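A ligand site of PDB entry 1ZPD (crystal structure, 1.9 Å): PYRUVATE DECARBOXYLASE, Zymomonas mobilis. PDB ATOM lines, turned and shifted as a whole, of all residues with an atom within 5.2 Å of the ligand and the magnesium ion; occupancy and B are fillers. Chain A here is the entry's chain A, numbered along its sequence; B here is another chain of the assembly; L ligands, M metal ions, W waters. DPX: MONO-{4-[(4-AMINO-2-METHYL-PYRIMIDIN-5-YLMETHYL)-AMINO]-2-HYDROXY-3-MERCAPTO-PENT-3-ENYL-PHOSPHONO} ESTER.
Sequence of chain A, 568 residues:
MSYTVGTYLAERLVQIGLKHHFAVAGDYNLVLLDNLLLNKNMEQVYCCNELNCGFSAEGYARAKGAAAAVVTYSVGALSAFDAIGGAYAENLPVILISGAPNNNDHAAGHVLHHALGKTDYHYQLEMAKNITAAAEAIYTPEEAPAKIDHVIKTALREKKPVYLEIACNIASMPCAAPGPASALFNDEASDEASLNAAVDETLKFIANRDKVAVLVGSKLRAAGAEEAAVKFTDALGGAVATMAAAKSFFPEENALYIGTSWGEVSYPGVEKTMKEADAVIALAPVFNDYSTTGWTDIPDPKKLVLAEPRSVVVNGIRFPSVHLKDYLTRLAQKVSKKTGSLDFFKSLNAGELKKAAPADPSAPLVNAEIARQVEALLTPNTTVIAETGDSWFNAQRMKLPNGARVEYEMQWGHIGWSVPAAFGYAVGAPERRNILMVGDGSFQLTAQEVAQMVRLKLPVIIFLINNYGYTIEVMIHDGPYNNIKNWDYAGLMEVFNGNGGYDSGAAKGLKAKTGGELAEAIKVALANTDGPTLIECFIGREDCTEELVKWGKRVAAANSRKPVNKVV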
ATOM      1  N   GLU A 387       3.105   2.055  -7.399  1.00  0.00           N
ATOM      2  CA  GLU A 387       1.933   1.175  -7.210  1.00  0.00           C
ATOM      3  C   GLU A 387       0.674   1.973  -6.932  1.00  0.00           C
ATOM      4  O   GLU A 387       0.682   3.031  -6.286  1.00  0.00           O
ATOM      5  CB  GLU A 387       2.197   0.246  -6.013  1.00  0.00           C
ATOM      6  CG  GLU A 387       1.099  -0.803  -5.724  1.00  0.00           C
ATOM      7  CD  GLU A 387       0.870  -1.760  -6.886  1.00  0.00           C
ATOM      8  OE1 GLU A 387       0.138  -1.381  -7.824  1.00  0.00           O
ATOM      9  OE2 GLU A 387       1.428  -2.876  -6.880  1.00  0.00           O
ATOM     10  N   THR A 388      -0.457   1.388  -7.357  1.00  0.00           N
ATOM     11  CA  THR A 388      -1.772   1.844  -6.922  1.00  0.00           C
ATOM     12  C   THR A 388      -1.821   1.942  -5.388  1.00  0.00           C
ATOM     13  O   THR A 388      -1.543   0.974  -4.658  1.00  0.00           O
ATOM     14  CB  THR A 388      -2.898   0.900  -7.419  1.00  0.00           C
ATOM     15  OG1 THR A 388      -2.892   0.912  -8.868  1.00  0.00           O
ATOM     16  CG2 THR A 388      -4.260   1.366  -6.918  1.00  0.00           C
ATOM     17  N   GLY A 389      -2.221   3.098  -4.923  1.00  0.00           N
ATOM     18  CA  GLY A 389      -2.276   3.397  -3.480  1.00  0.00           C
ATOM     19  C   GLY A 389      -1.785   4.841  -3.286  1.00  0.00           C
ATOM     20  O   GLY A 389      -1.710   5.580  -4.280  1.00  0.00           O
ATOM     21  N   ASP A 390      -1.402   5.229  -2.059  1.00  0.00           N
ATOM     22  CA  ASP A 390      -0.902   6.613  -1.881  1.00  0.00           C
ATOM     23  C   ASP A 390       0.408   6.859  -2.618  1.00  0.00           C
ATOM     24  O   ASP A 390       0.734   8.018  -2.940  1.00  0.00           O
ATOM     25  CB  ASP A 390      -0.802   7.011  -0.408  1.00  0.00           C
ATOM     26  CG  ASP A 390      -0.853   8.524  -0.221  1.00  0.00           C
ATOM     27  OD1 ASP A 390      -1.498   9.274  -1.003  1.00  0.00           O
ATOM     28  OD2 ASP A 390      -0.232   8.997   0.766  1.00  0.00           O
ATOM     29  N   SER A 391       1.142   5.826  -2.982  1.00  0.00           N
ATOM     30  CA  SER A 391       2.328   5.939  -3.835  1.00  0.00           C
ATOM     31  C   SER A 391       1.993   6.588  -5.190  1.00  0.00           C
ATOM     32  O   SER A 391       2.916   7.184  -5.769  1.00  0.00           O
ATOM     33  CB  SER A 391       2.985   4.580  -4.075  1.00  0.00           C
ATOM     34  OG  SER A 391       3.572   4.037  -2.908  1.00  0.00           O
ATOM     35  N   GLY A 413      -5.063  -0.709 -12.721  1.00  0.00           N
ATOM     36  CA  GLY A 413      -5.015  -0.515 -11.276  1.00  0.00           C
ATOM     37  C   GLY A 413      -5.160  -1.792 -10.446  1.00  0.00           C
ATOM     38  O   GLY A 413      -5.892  -1.800  -9.447  1.00  0.00           O
ATOM     39  N   HIS A 414      -4.460  -2.852 -10.812  1.00  0.00           N
ATOM     40  CA  HIS A 414      -4.452  -4.096 -10.053  1.00  0.00           C
ATOM     41  C   HIS A 414      -3.393  -4.016  -8.944  1.00  0.00           C
ATOM     42  O   HIS A 414      -2.194  -4.059  -9.281  1.00  0.00           O
ATOM     43  CB  HIS A 414      -4.152  -5.265 -10.987  1.00  0.00           C
ATOM     44  CG  HIS A 414      -4.137  -6.641 -10.389  1.00  0.00           C
ATOM     45  ND1 HIS A 414      -3.322  -6.994  -9.327  1.00  0.00           N
ATOM     46  CD2 HIS A 414      -4.858  -7.757 -10.707  1.00  0.00           C
ATOM     47  CE1 HIS A 414      -3.542  -8.273  -9.018  1.00  0.00           C
ATOM     48  NE2 HIS A 414      -4.477  -8.759  -9.828  1.00  0.00           N
ATOM     49  N   ILE A 415      -3.816  -3.861  -7.681  1.00  0.00           N
ATOM     50  CA  ILE A 415      -2.809  -3.732  -6.607  1.00  0.00           C
ATOM     51  C   ILE A 415      -1.965  -5.001  -6.611  1.00  0.00           C
ATOM     52  O   ILE A 415      -2.425  -6.124  -6.887  1.00  0.00           O
ATOM     53  CB  ILE A 415      -3.369  -3.442  -5.202  1.00  0.00           C
ATOM     54  CG1 ILE A 415      -4.355  -4.557  -4.764  1.00  0.00           C
ATOM     55  CG2 ILE A 415      -4.030  -2.069  -5.146  1.00  0.00           C
ATOM     56  CD1 ILE A 415      -4.595  -4.511  -3.247  1.00  0.00           C
ATOM     57  N   GLY A 439       2.927  -0.108  -1.529  1.00  0.00           N
ATOM     58  CA  GLY A 439       2.320  -0.175  -0.208  1.00  0.00           C
ATOM     59  C   GLY A 439       2.274  -1.597   0.341  1.00  0.00           C
ATOM     60  O   GLY A 439       2.383  -2.564  -0.416  1.00  0.00           O
ATOM     61  N   ASP A 440       2.079  -1.743   1.657  1.00  0.00           N
ATOM     62  CA  ASP A 440       2.024  -3.057   2.309  1.00  0.00           C
ATOM     63  C   ASP A 440       0.878  -3.927   1.779  1.00  0.00           C
ATOM     64  O   ASP A 440       1.095  -5.115   1.519  1.00  0.00           O
ATOM     65  CB  ASP A 440       1.886  -2.895   3.838  1.00  0.00           C
ATOM     66  CG  ASP A 440       0.758  -2.016   4.308  1.00  0.00           C
ATOM     67  OD1 ASP A 440       0.250  -1.107   3.621  1.00  0.00           O
ATOM     68  OD2 ASP A 440       0.321  -2.220   5.474  1.00  0.00           O
ATOM     69  N   GLY A 441      -0.310  -3.344   1.620  1.00  0.00           N
ATOM     70  CA  GLY A 441      -1.461  -4.142   1.140  1.00  0.00           C
ATOM     71  C   GLY A 441      -1.220  -4.730  -0.240  1.00  0.00           C
ATOM     72  O   GLY A 441      -1.461  -5.929  -0.471  1.00  0.00           O
ATOM     73  N   SER A 442      -0.742  -3.887  -1.177  1.00  0.00           N
ATOM     74  CA  SER A 442      -0.437  -4.348  -2.527  1.00  0.00           C
ATOM     75  C   SER A 442       0.661  -5.397  -2.531  1.00  0.00           C
ATOM     76  O   SER A 442       0.569  -6.386  -3.272  1.00  0.00           O
ATOM     77  CB  SER A 442       0.028  -3.164  -3.413  1.00  0.00           C
ATOM     78  OG  SER A 442      -0.962  -2.157  -3.498  1.00  0.00           O
ATOM     79  N   PHE A 443       1.714  -5.183  -1.726  1.00  0.00           N
ATOM     80  CA  PHE A 443       2.852  -6.084  -1.695  1.00  0.00           C
ATOM     81  C   PHE A 443       2.441  -7.531  -1.437  1.00  0.00           C
ATOM     82  O   PHE A 443       2.959  -8.469  -2.032  1.00  0.00           O
ATOM     83  CB  PHE A 443       3.871  -5.626  -0.628  1.00  0.00           C
ATOM     84  CG  PHE A 443       5.194  -6.350  -0.632  1.00  0.00           C
ATOM     85  CD1 PHE A 443       6.149  -6.079  -1.599  1.00  0.00           C
ATOM     86  CD2 PHE A 443       5.499  -7.270   0.362  1.00  0.00           C
ATOM     87  CE1 PHE A 443       7.365  -6.742  -1.589  1.00  0.00           C
ATOM     88  CE2 PHE A 443       6.702  -7.946   0.386  1.00  0.00           C
ATOM     89  CZ  PHE A 443       7.650  -7.671  -0.599  1.00  0.00           C
ATOM     90  N   LEU A 445      -0.101  -9.225  -2.389  1.00  0.00           N
ATOM     91  CA  LEU A 445      -0.728 -10.023  -3.459  1.00  0.00           C
ATOM     92  C   LEU A 445       0.268 -10.794  -4.294  1.00  0.00           C
ATOM     93  O   LEU A 445      -0.026 -11.850  -4.883  1.00  0.00           O
ATOM     94  CB  LEU A 445      -1.582  -9.149  -4.392  1.00  0.00           C
ATOM     95  CG  LEU A 445      -2.969  -8.772  -3.876  1.00  0.00           C
ATOM     96  CD1 LEU A 445      -2.895  -7.488  -3.036  1.00  0.00           C
ATOM     97  CD2 LEU A 445      -3.945  -8.578  -5.033  1.00  0.00           C
ATOM     98  N   ILE A 465       5.869   0.765   1.944  1.00  0.00           N
ATOM     99  CA  ILE A 465       5.223   1.762   2.794  1.00  0.00           C
ATOM    100  C   ILE A 465       4.307   1.032   3.798  1.00  0.00           C
ATOM    101  O   ILE A 465       3.196   0.615   3.420  1.00  0.00           O
ATOM    102  CB  ILE A 465       4.474   2.820   1.975  1.00  0.00           C
ATOM    103  CG1 ILE A 465       5.327   3.350   0.804  1.00  0.00           C
ATOM    104  CG2 ILE A 465       4.011   3.982   2.844  1.00  0.00           C
ATOM    105  CD1 ILE A 465       6.680   3.952   1.192  1.00  0.00           C
ATOM    106  N   ASN A 467       1.979   1.297   6.390  1.00  0.00           N
ATOM    107  CA  ASN A 467       0.984   2.043   7.142  1.00  0.00           C
ATOM    108  C   ASN A 467      -0.111   1.094   7.682  1.00  0.00           C
ATOM    109  O   ASN A 467      -1.200   1.555   8.031  1.00  0.00           O
ATOM    110  CB  ASN A 467       0.390   3.160   6.278  1.00  0.00           C
ATOM    111  CG  ASN A 467      -0.203   2.709   4.952  1.00  0.00           C
ATOM    112  OD1 ASN A 467      -0.395   1.509   4.722  1.00  0.00           O
ATOM    113  ND2 ASN A 467      -0.531   3.643   4.070  1.00  0.00           N
ATOM    114  N   TYR A 468       0.157  -0.197   7.734  1.00  0.00           N
ATOM    115  CA  TYR A 468      -0.759  -1.182   8.344  1.00  0.00           C
ATOM    116  C   TYR A 468      -2.151  -1.150   7.722  1.00  0.00           C
ATOM    117  O   TYR A 468      -3.130  -0.917   8.443  1.00  0.00           O
ATOM    118  CB  TYR A 468      -0.787  -1.023   9.870  1.00  0.00           C
ATOM    119  CG  TYR A 468      -1.327  -2.214  10.654  1.00  0.00           C
ATOM    120  CD1 TYR A 468      -1.116  -3.533  10.272  1.00  0.00           C
ATOM    121  CD2 TYR A 468      -2.078  -1.997  11.806  1.00  0.00           C
ATOM    122  CE1 TYR A 468      -1.627  -4.604  11.000  1.00  0.00           C
ATOM    123  CE2 TYR A 468      -2.597  -3.060  12.562  1.00  0.00           C
ATOM    124  CZ  TYR A 468      -2.361  -4.355  12.151  1.00  0.00           C
ATOM    125  OH  TYR A 468      -2.875  -5.418  12.883  1.00  0.00           O
ATOM    126  N   GLY A 469      -2.255  -1.439   6.415  1.00  0.00           N
ATOM    127  CA  GLY A 469      -3.594  -1.624   5.805  1.00  0.00           C
ATOM    128  C   GLY A 469      -3.757  -0.858   4.488  1.00  0.00           C
ATOM    129  O   GLY A 469      -2.806  -0.301   3.922  1.00  0.00           O
ATOM    130  N   TYR A 470      -5.005  -0.740   4.031  1.00  0.00           N
ATOM    131  CA  TYR A 470      -5.320  -0.137   2.725  1.00  0.00           C
ATOM    132  C   TYR A 470      -5.722   1.330   2.865  1.00  0.00           C
ATOM    133  O   TYR A 470      -6.918   1.647   2.856  1.00  0.00           O
ATOM    134  CB  TYR A 470      -6.454  -0.926   2.041  1.00  0.00           C
ATOM    135  CG  TYR A 470      -6.327  -2.396   1.753  1.00  0.00           C
ATOM    136  CD1 TYR A 470      -5.121  -3.014   1.466  1.00  0.00           C
ATOM    137  CD2 TYR A 470      -7.471  -3.205   1.744  1.00  0.00           C
ATOM    138  CE1 TYR A 470      -5.043  -4.366   1.179  1.00  0.00           C
ATOM    139  CE2 TYR A 470      -7.413  -4.573   1.473  1.00  0.00           C
ATOM    140  CZ  TYR A 470      -6.195  -5.151   1.189  1.00  0.00           C
ATOM    141  OH  TYR A 470      -6.150  -6.501   0.916  1.00  0.00           O
ATOM    142  N   THR A 471      -4.755   2.268   2.954  1.00  0.00           N
ATOM    143  CA  THR A 471      -5.104   3.655   3.265  1.00  0.00           C
ATOM    144  C   THR A 471      -5.938   4.298   2.168  1.00  0.00           C
ATOM    145  O   THR A 471      -6.887   5.022   2.476  1.00  0.00           O
ATOM    146  CB  THR A 471      -3.828   4.485   3.586  1.00  0.00           C
ATOM    147  OG1 THR A 471      -3.427   4.163   4.944  1.00  0.00           O
ATOM    148  CG2 THR A 471      -4.053   5.993   3.515  1.00  0.00           C
ATOM    149  N   ILE A 472      -5.613   4.077   0.890  1.00  0.00           N
ATOM    150  CA  ILE A 472      -6.423   4.674  -0.182  1.00  0.00           C
ATOM    151  C   ILE A 472      -7.871   4.200  -0.072  1.00  0.00           C
ATOM    152  O   ILE A 472      -8.770   5.020  -0.199  1.00  0.00           O
ATOM    153  CB  ILE A 472      -5.875   4.380  -1.593  1.00  0.00           C
ATOM    154  CG1 ILE A 472      -6.763   5.022  -2.667  1.00  0.00           C
ATOM    155  CG2 ILE A 472      -5.761   2.883  -1.859  1.00  0.00           C
ATOM    156  CD1 ILE A 472      -7.788   4.076  -3.274  1.00  0.00           C
ATOM    157  N   GLU A 473      -8.140   2.922   0.236  1.00  0.00           N
ATOM    158  CA  GLU A 473      -9.497   2.435   0.459  1.00  0.00           C
ATOM    159  C   GLU A 473     -10.139   3.020   1.713  1.00  0.00           C
ATOM    160  O   GLU A 473     -11.302   3.438   1.699  1.00  0.00           O
ATOM    161  CB  GLU A 473      -9.503   0.895   0.503  1.00  0.00           C
ATOM    162  CG  GLU A 473     -10.652   0.225  -0.229  1.00  0.00           C
ATOM    163  CD  GLU A 473     -10.514   0.246  -1.745  1.00  0.00           C
ATOM    164  OE1 GLU A 473     -10.296   1.317  -2.359  1.00  0.00           O
ATOM    165  OE2 GLU A 473     -10.642  -0.852  -2.348  1.00  0.00           O
ATOM    166  N   VAL B  24     -12.059 -10.039  -0.774  1.00  0.00           N
ATOM    167  CA  VAL B  24     -10.945  -9.056  -0.906  1.00  0.00           C
ATOM    168  C   VAL B  24     -11.600  -7.729  -1.315  1.00  0.00           C
ATOM    169  O   VAL B  24     -12.285  -7.631  -2.350  1.00  0.00           O
ATOM    170  CB  VAL B  24      -9.886  -9.403  -1.950  1.00  0.00           C
ATOM    171  CG1 VAL B  24      -8.830  -8.260  -1.992  1.00  0.00           C
ATOM    172  CG2 VAL B  24      -9.215 -10.732  -1.692  1.00  0.00           C
ATOM    173  N   ALA B  25     -11.433  -6.686  -0.496  1.00  0.00           N
ATOM    174  CA  ALA B  25     -12.044  -5.399  -0.722  1.00  0.00           C
ATOM    175  C   ALA B  25     -11.575  -4.729  -2.032  1.00  0.00           C
ATOM    176  O   ALA B  25     -10.446  -4.898  -2.495  1.00  0.00           O
ATOM    177  CB  ALA B  25     -11.720  -4.441   0.433  1.00  0.00           C
ATOM    178  N   GLY B  26     -12.477  -3.961  -2.588  1.00  0.00           N
ATOM    179  CA  GLY B  26     -12.232  -3.063  -3.734  1.00  0.00           C
ATOM    180  C   GLY B  26     -13.365  -2.066  -3.792  1.00  0.00           C
ATOM    181  O   GLY B  26     -14.473  -2.435  -3.354  1.00  0.00           O
ATOM    182  N   ASP B  27     -13.167  -0.873  -4.384  1.00  0.00           N
ATOM    183  CA  ASP B  27     -14.205   0.153  -4.311  1.00  0.00           C
ATOM    184  C   ASP B  27     -15.532  -0.285  -4.954  1.00  0.00           C
ATOM    185  O   ASP B  27     -16.582   0.187  -4.498  1.00  0.00           O
ATOM    186  CB  ASP B  27     -13.706   1.476  -4.886  1.00  0.00           C
ATOM    187  CG  ASP B  27     -13.292   1.530  -6.348  1.00  0.00           C
ATOM    188  OD1 ASP B  27     -13.087   0.467  -6.988  1.00  0.00           O
ATOM    189  OD2 ASP B  27     -13.170   2.680  -6.839  1.00  0.00           O
ATOM    190  N   GLU B  50      -7.051 -12.477  -4.869  1.00  0.00           N
ATOM    191  CA  GLU B  50      -8.321 -13.073  -5.291  1.00  0.00           C
ATOM    192  C   GLU B  50      -8.202 -14.505  -5.767  1.00  0.00           C
ATOM    193  O   GLU B  50      -9.192 -15.278  -5.680  1.00  0.00           O
ATOM    194  CB  GLU B  50      -8.996 -12.149  -6.334  1.00  0.00           C
ATOM    195  CG  GLU B  50      -9.456 -10.820  -5.754  1.00  0.00           C
ATOM    196  CD  GLU B  50      -8.405  -9.700  -5.776  1.00  0.00           C
ATOM    197  OE1 GLU B  50      -7.259  -9.991  -6.151  1.00  0.00           O
ATOM    198  OE2 GLU B  50      -8.750  -8.544  -5.446  1.00  0.00           O
ATOM    199  N   THR B  72     -13.585  -7.720  -6.377  1.00  0.00           N
ATOM    200  CA  THR B  72     -13.888  -6.486  -7.089  1.00  0.00           C
ATOM    201  C   THR B  72     -13.913  -6.711  -8.604  1.00  0.00           C
ATOM    202  O   THR B  72     -13.340  -7.687  -9.098  1.00  0.00           O
ATOM    203  CB  THR B  72     -12.960  -5.312  -6.694  1.00  0.00           C
ATOM    204  OG1 THR B  72     -13.567  -4.087  -7.111  1.00  0.00           O
ATOM    205  CG2 THR B  72     -11.578  -5.434  -7.346  1.00  0.00           C
ATOM    206  N   VAL B  75     -10.216  -6.700 -12.197  1.00  0.00           N
ATOM    207  CA  VAL B  75      -8.939  -7.038 -11.574  1.00  0.00           C
ATOM    208  C   VAL B  75      -9.106  -8.075 -10.455  1.00  0.00           C
ATOM    209  O   VAL B  75      -8.156  -8.827 -10.260  1.00  0.00           O
ATOM    210  CB  VAL B  75      -8.202  -5.779 -11.036  1.00  0.00           C
ATOM    211  CG1 VAL B  75      -7.850  -4.824 -12.195  1.00  0.00           C
ATOM    212  CG2 VAL B  75      -9.003  -5.037  -9.981  1.00  0.00           C
ATOM    213  N   GLY B  76     -10.244  -8.120  -9.742  1.00  0.00           N
ATOM    214  CA  GLY B  76     -10.421  -9.190  -8.758  1.00  0.00           C
ATOM    215  C   GLY B  76     -11.059 -10.461  -9.352  1.00  0.00           C
ATOM    216  O   GLY B  76     -10.624 -11.586  -9.096  1.00  0.00           O
ATOM    217  N   HIS B 114     -10.283  -0.186 -13.811  1.00  0.00           N
ATOM    218  CA  HIS B 114     -10.229  -1.638 -13.710  1.00  0.00           C
ATOM    219  C   HIS B 114     -10.722  -2.375 -14.970  1.00  0.00           C
ATOM    220  O   HIS B 114     -10.530  -3.614 -15.019  1.00  0.00           O
ATOM    221  CB  HIS B 114     -10.965  -2.221 -12.500  1.00  0.00           C
ATOM    222  CG  HIS B 114     -10.459  -1.865 -11.133  1.00  0.00           C
ATOM    223  ND1 HIS B 114      -9.161  -1.459 -10.882  1.00  0.00           N
ATOM    224  CD2 HIS B 114     -11.092  -1.887  -9.924  1.00  0.00           C
ATOM    225  CE1 HIS B 114      -9.025  -1.208  -9.586  1.00  0.00           C
ATOM    226  NE2 HIS B 114     -10.169  -1.467  -8.967  1.00  0.00           N
HETATM  227  C4  DPX L   1      -7.124  -1.717  -2.849  1.00  0.00           C
HETATM  228  C5  DPX L   1      -6.212  -0.727  -2.516  1.00  0.00           C
HETATM  229  O21 DPX L   1      -1.382  -0.835   1.246  1.00  0.00           O
HETATM  230  O22 DPX L   1      -1.623   1.281  -0.215  1.00  0.00           O
HETATM  231  O26 DPX L   1      -3.356   2.857   0.088  1.00  0.00           O
HETATM  232  O25 DPX L   1      -1.133   3.723   0.241  1.00  0.00           O
HETATM  233  O24 DPX L   1      -1.950   2.094   1.966  1.00  0.00           O
HETATM  234  P23 DPX L   1      -1.973   2.587   0.557  1.00  0.00           P
HETATM  235  P19 DPX L   1      -1.644  -0.319  -0.100  1.00  0.00           P
HETATM  236  O20 DPX L   1      -0.945  -1.039  -1.128  1.00  0.00           O
HETATM  237  O18 DPX L   1      -3.237  -0.730  -0.258  1.00  0.00           O
HETATM  238  C17 DPX L   1      -3.872  -0.543  -1.541  1.00  0.00           C
HETATM  239  C16 DPX L   1      -5.360  -0.565  -1.247  1.00  0.00           C
HETATM  240  C15 DPX L   1      -7.442  -2.895  -1.947  1.00  0.00           C
HETATM  241  N3  DPX L   1      -7.716  -1.600  -4.053  1.00  0.00           N
HETATM  242  S1  DPX L   1      -6.063   0.536  -3.715  1.00  0.00           S
HETATM  243  C6  DPX L   1      -8.767  -2.617  -4.574  1.00  0.00           C
HETATM  244  C7  DPX L   1      -8.176  -3.765  -5.353  1.00  0.00           C
HETATM  245  C8  DPX L   1      -7.411  -3.537  -6.589  1.00  0.00           C
HETATM  246  N9  DPX L   1      -6.887  -4.583  -7.263  1.00  0.00           N
HETATM  247  C10 DPX L   1      -7.045  -5.809  -6.805  1.00  0.00           C
HETATM  248  N11 DPX L   1      -7.908  -6.098  -5.771  1.00  0.00           N
HETATM  249  C12 DPX L   1      -8.336  -5.073  -4.987  1.00  0.00           C
HETATM  250  N13 DPX L   1      -7.221  -2.277  -7.032  1.00  0.00           N
HETATM  251  C14 DPX L   1      -6.468  -6.957  -7.511  1.00  0.00           C
HETATM  252 MG    MG M   1      -0.904   0.331   3.039  1.00  0.00          MG
HETATM  253  O   HOH W   1       1.322   3.056  -1.766  1.00  0.00           O
HETATM  254  O   HOH W   2      -8.214   0.452  -6.512  1.00  0.00           O
HETATM  255  O   HOH W   3       0.838   1.372   2.183  1.00  0.00           O
HETATM  256  O   HOH W   4       0.443   0.562  -2.795  1.00  0.00           O
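A nitrogen (N11) of the ligand lies within hydrogen-bond range of the side-chain carboxylate of Glu 50 of chain B (2.6 Å).
O20 of the ligand is in hydrogen-bond range of N of Ser 442, at 2.9 Å.
An oxygen (O20) of the ligand is in hydrogen-bond range of the side-chain hydroxyl (OG) of Ser 442, at 2.6 Å.
N of Ile 472 sits at hydrogen-bond distance from O26 of the ligand (2.7 Å).
The backbone NH (N) of Gly 441 lies close to an oxygen (O21) of the ligand.
N of Asp 390 sits at hydrogen-bond distance from O25 of the ligand.
O of Gly 413 sits at hydrogen-bond distance from N13 of the ligand (2.8 Å).
The backbone NH (N) of Thr 471 is in hydrogen-bond range of an oxygen (O26) of the ligand (3.2 Å).
N of Ile 415 sits at hydrogen-bond distance from N9 of the ligand (3.2 Å).
N3 of the ligand lies close to OE2 of Glu 473.
The backbone NH (N) of Asp 440 lies within hydrogen-bond range of the backbone carbonyl oxygen (O) of Ile 465, 3.1 Å away.
OD2 of Asp 440 is in hydrogen-bond range of N of Tyr 468 (3.0 Å).
OG1 of Thr 471 lies within hydrogen-bond range of ND2 of Asn 467.
The side-chain hydroxyl (OG) of Ser 442 sits at hydrogen-bond distance from the backbone carbonyl oxygen (O) of Thr 388 (3.4 Å).
The side-chain carboxylate (OE2) of Glu 473 is in hydrogen-bond range of the backbone NH (N) of Asp 27 of chain B (3.2 Å).
Thr 388 touches the ligand.
C of Gly 389 touches O25 of the ligand (3.8 Å).
His 414 touches the ligand.
Gly 439 touches the ligand.
Leu 445 touches the ligand.
Tyr 470 touches the ligand.
Ala 25 of chain B touches the ligand (O to C12, 3.3 Å).
Gly 26 of chain B touches the ligand.
CG2 of Val 75 of chain B touches N9 of the ligand, 3.5 Å away.
His 114 of chain B touches the ligand (CE1 to N13, 3.3 Å).
Hydrophobic or aromatic side chains within 4 Å of the ligand: His 414, Ile 415, Leu 445, Tyr 470, Ile 472, Val 75 of chain B and His 114 of chain B.
22 residues have an atom within 4 Å of the ligand: Thr 388, Gly 389, Asp 390, Gly 413, His 414, Ile 415, Gly 439, Asp 440, Gly 441, Ser 442, Leu 445, Asn 467, Gly 469, Tyr 470, Thr 471, Ile 472, Glu 473, Ala 25 of chain B, Gly 26 of chain B, Glu 50 of chain B, Val 75 of chain B and His 114 of chain B.
The nearest printed residue that does not touch the ligand is Thr 72 of chain B (4.03 Å).
Merely in contact with the magnesium ion: Gly 441 (3.98 Å).
OD1 of Asp 440 is bound to the magnesium ion, 1.9 Å away.
The side-chain amide oxygen (OD1) of Asn 467 is bound to the magnesium ion, at 2.1 Å.
The backbone carbonyl oxygen (O) of Gly 469 binds the magnesium ion (2.2 Å).
An oxygen (O21) of the ligand binds the magnesium ion (2.2 Å).
Water W3 is bound to the magnesium ion.
An oxygen (O24) of the ligand is bound to the magnesium ion (2.3 Å).
The magnesium ion has six donor atoms within binding distance.
Water W3 lies within hydrogen-bond range of O of Ile 465 (2.8 Å), ND2 of Asn 467 (3.3 Å), N of Asp 440 (3.4 Å) and O22 of the ligand (3.4 Å).
Water W4 lies within hydrogen-bond range of an oxygen (O20) of the ligand (2.7 Å), the backbone carbonyl oxygen of Thr 388 (2.8 Å), the backbone NH of Gly 439 (2.9 Å) and the side-chain hydroxyl of Ser 442 (3.1 Å).
Water W1 lies within hydrogen-bond range of OG of Ser 391 (2.7 Å), O25 of the ligand (3.2 Å) and N of Asp 390 (3.5 Å).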
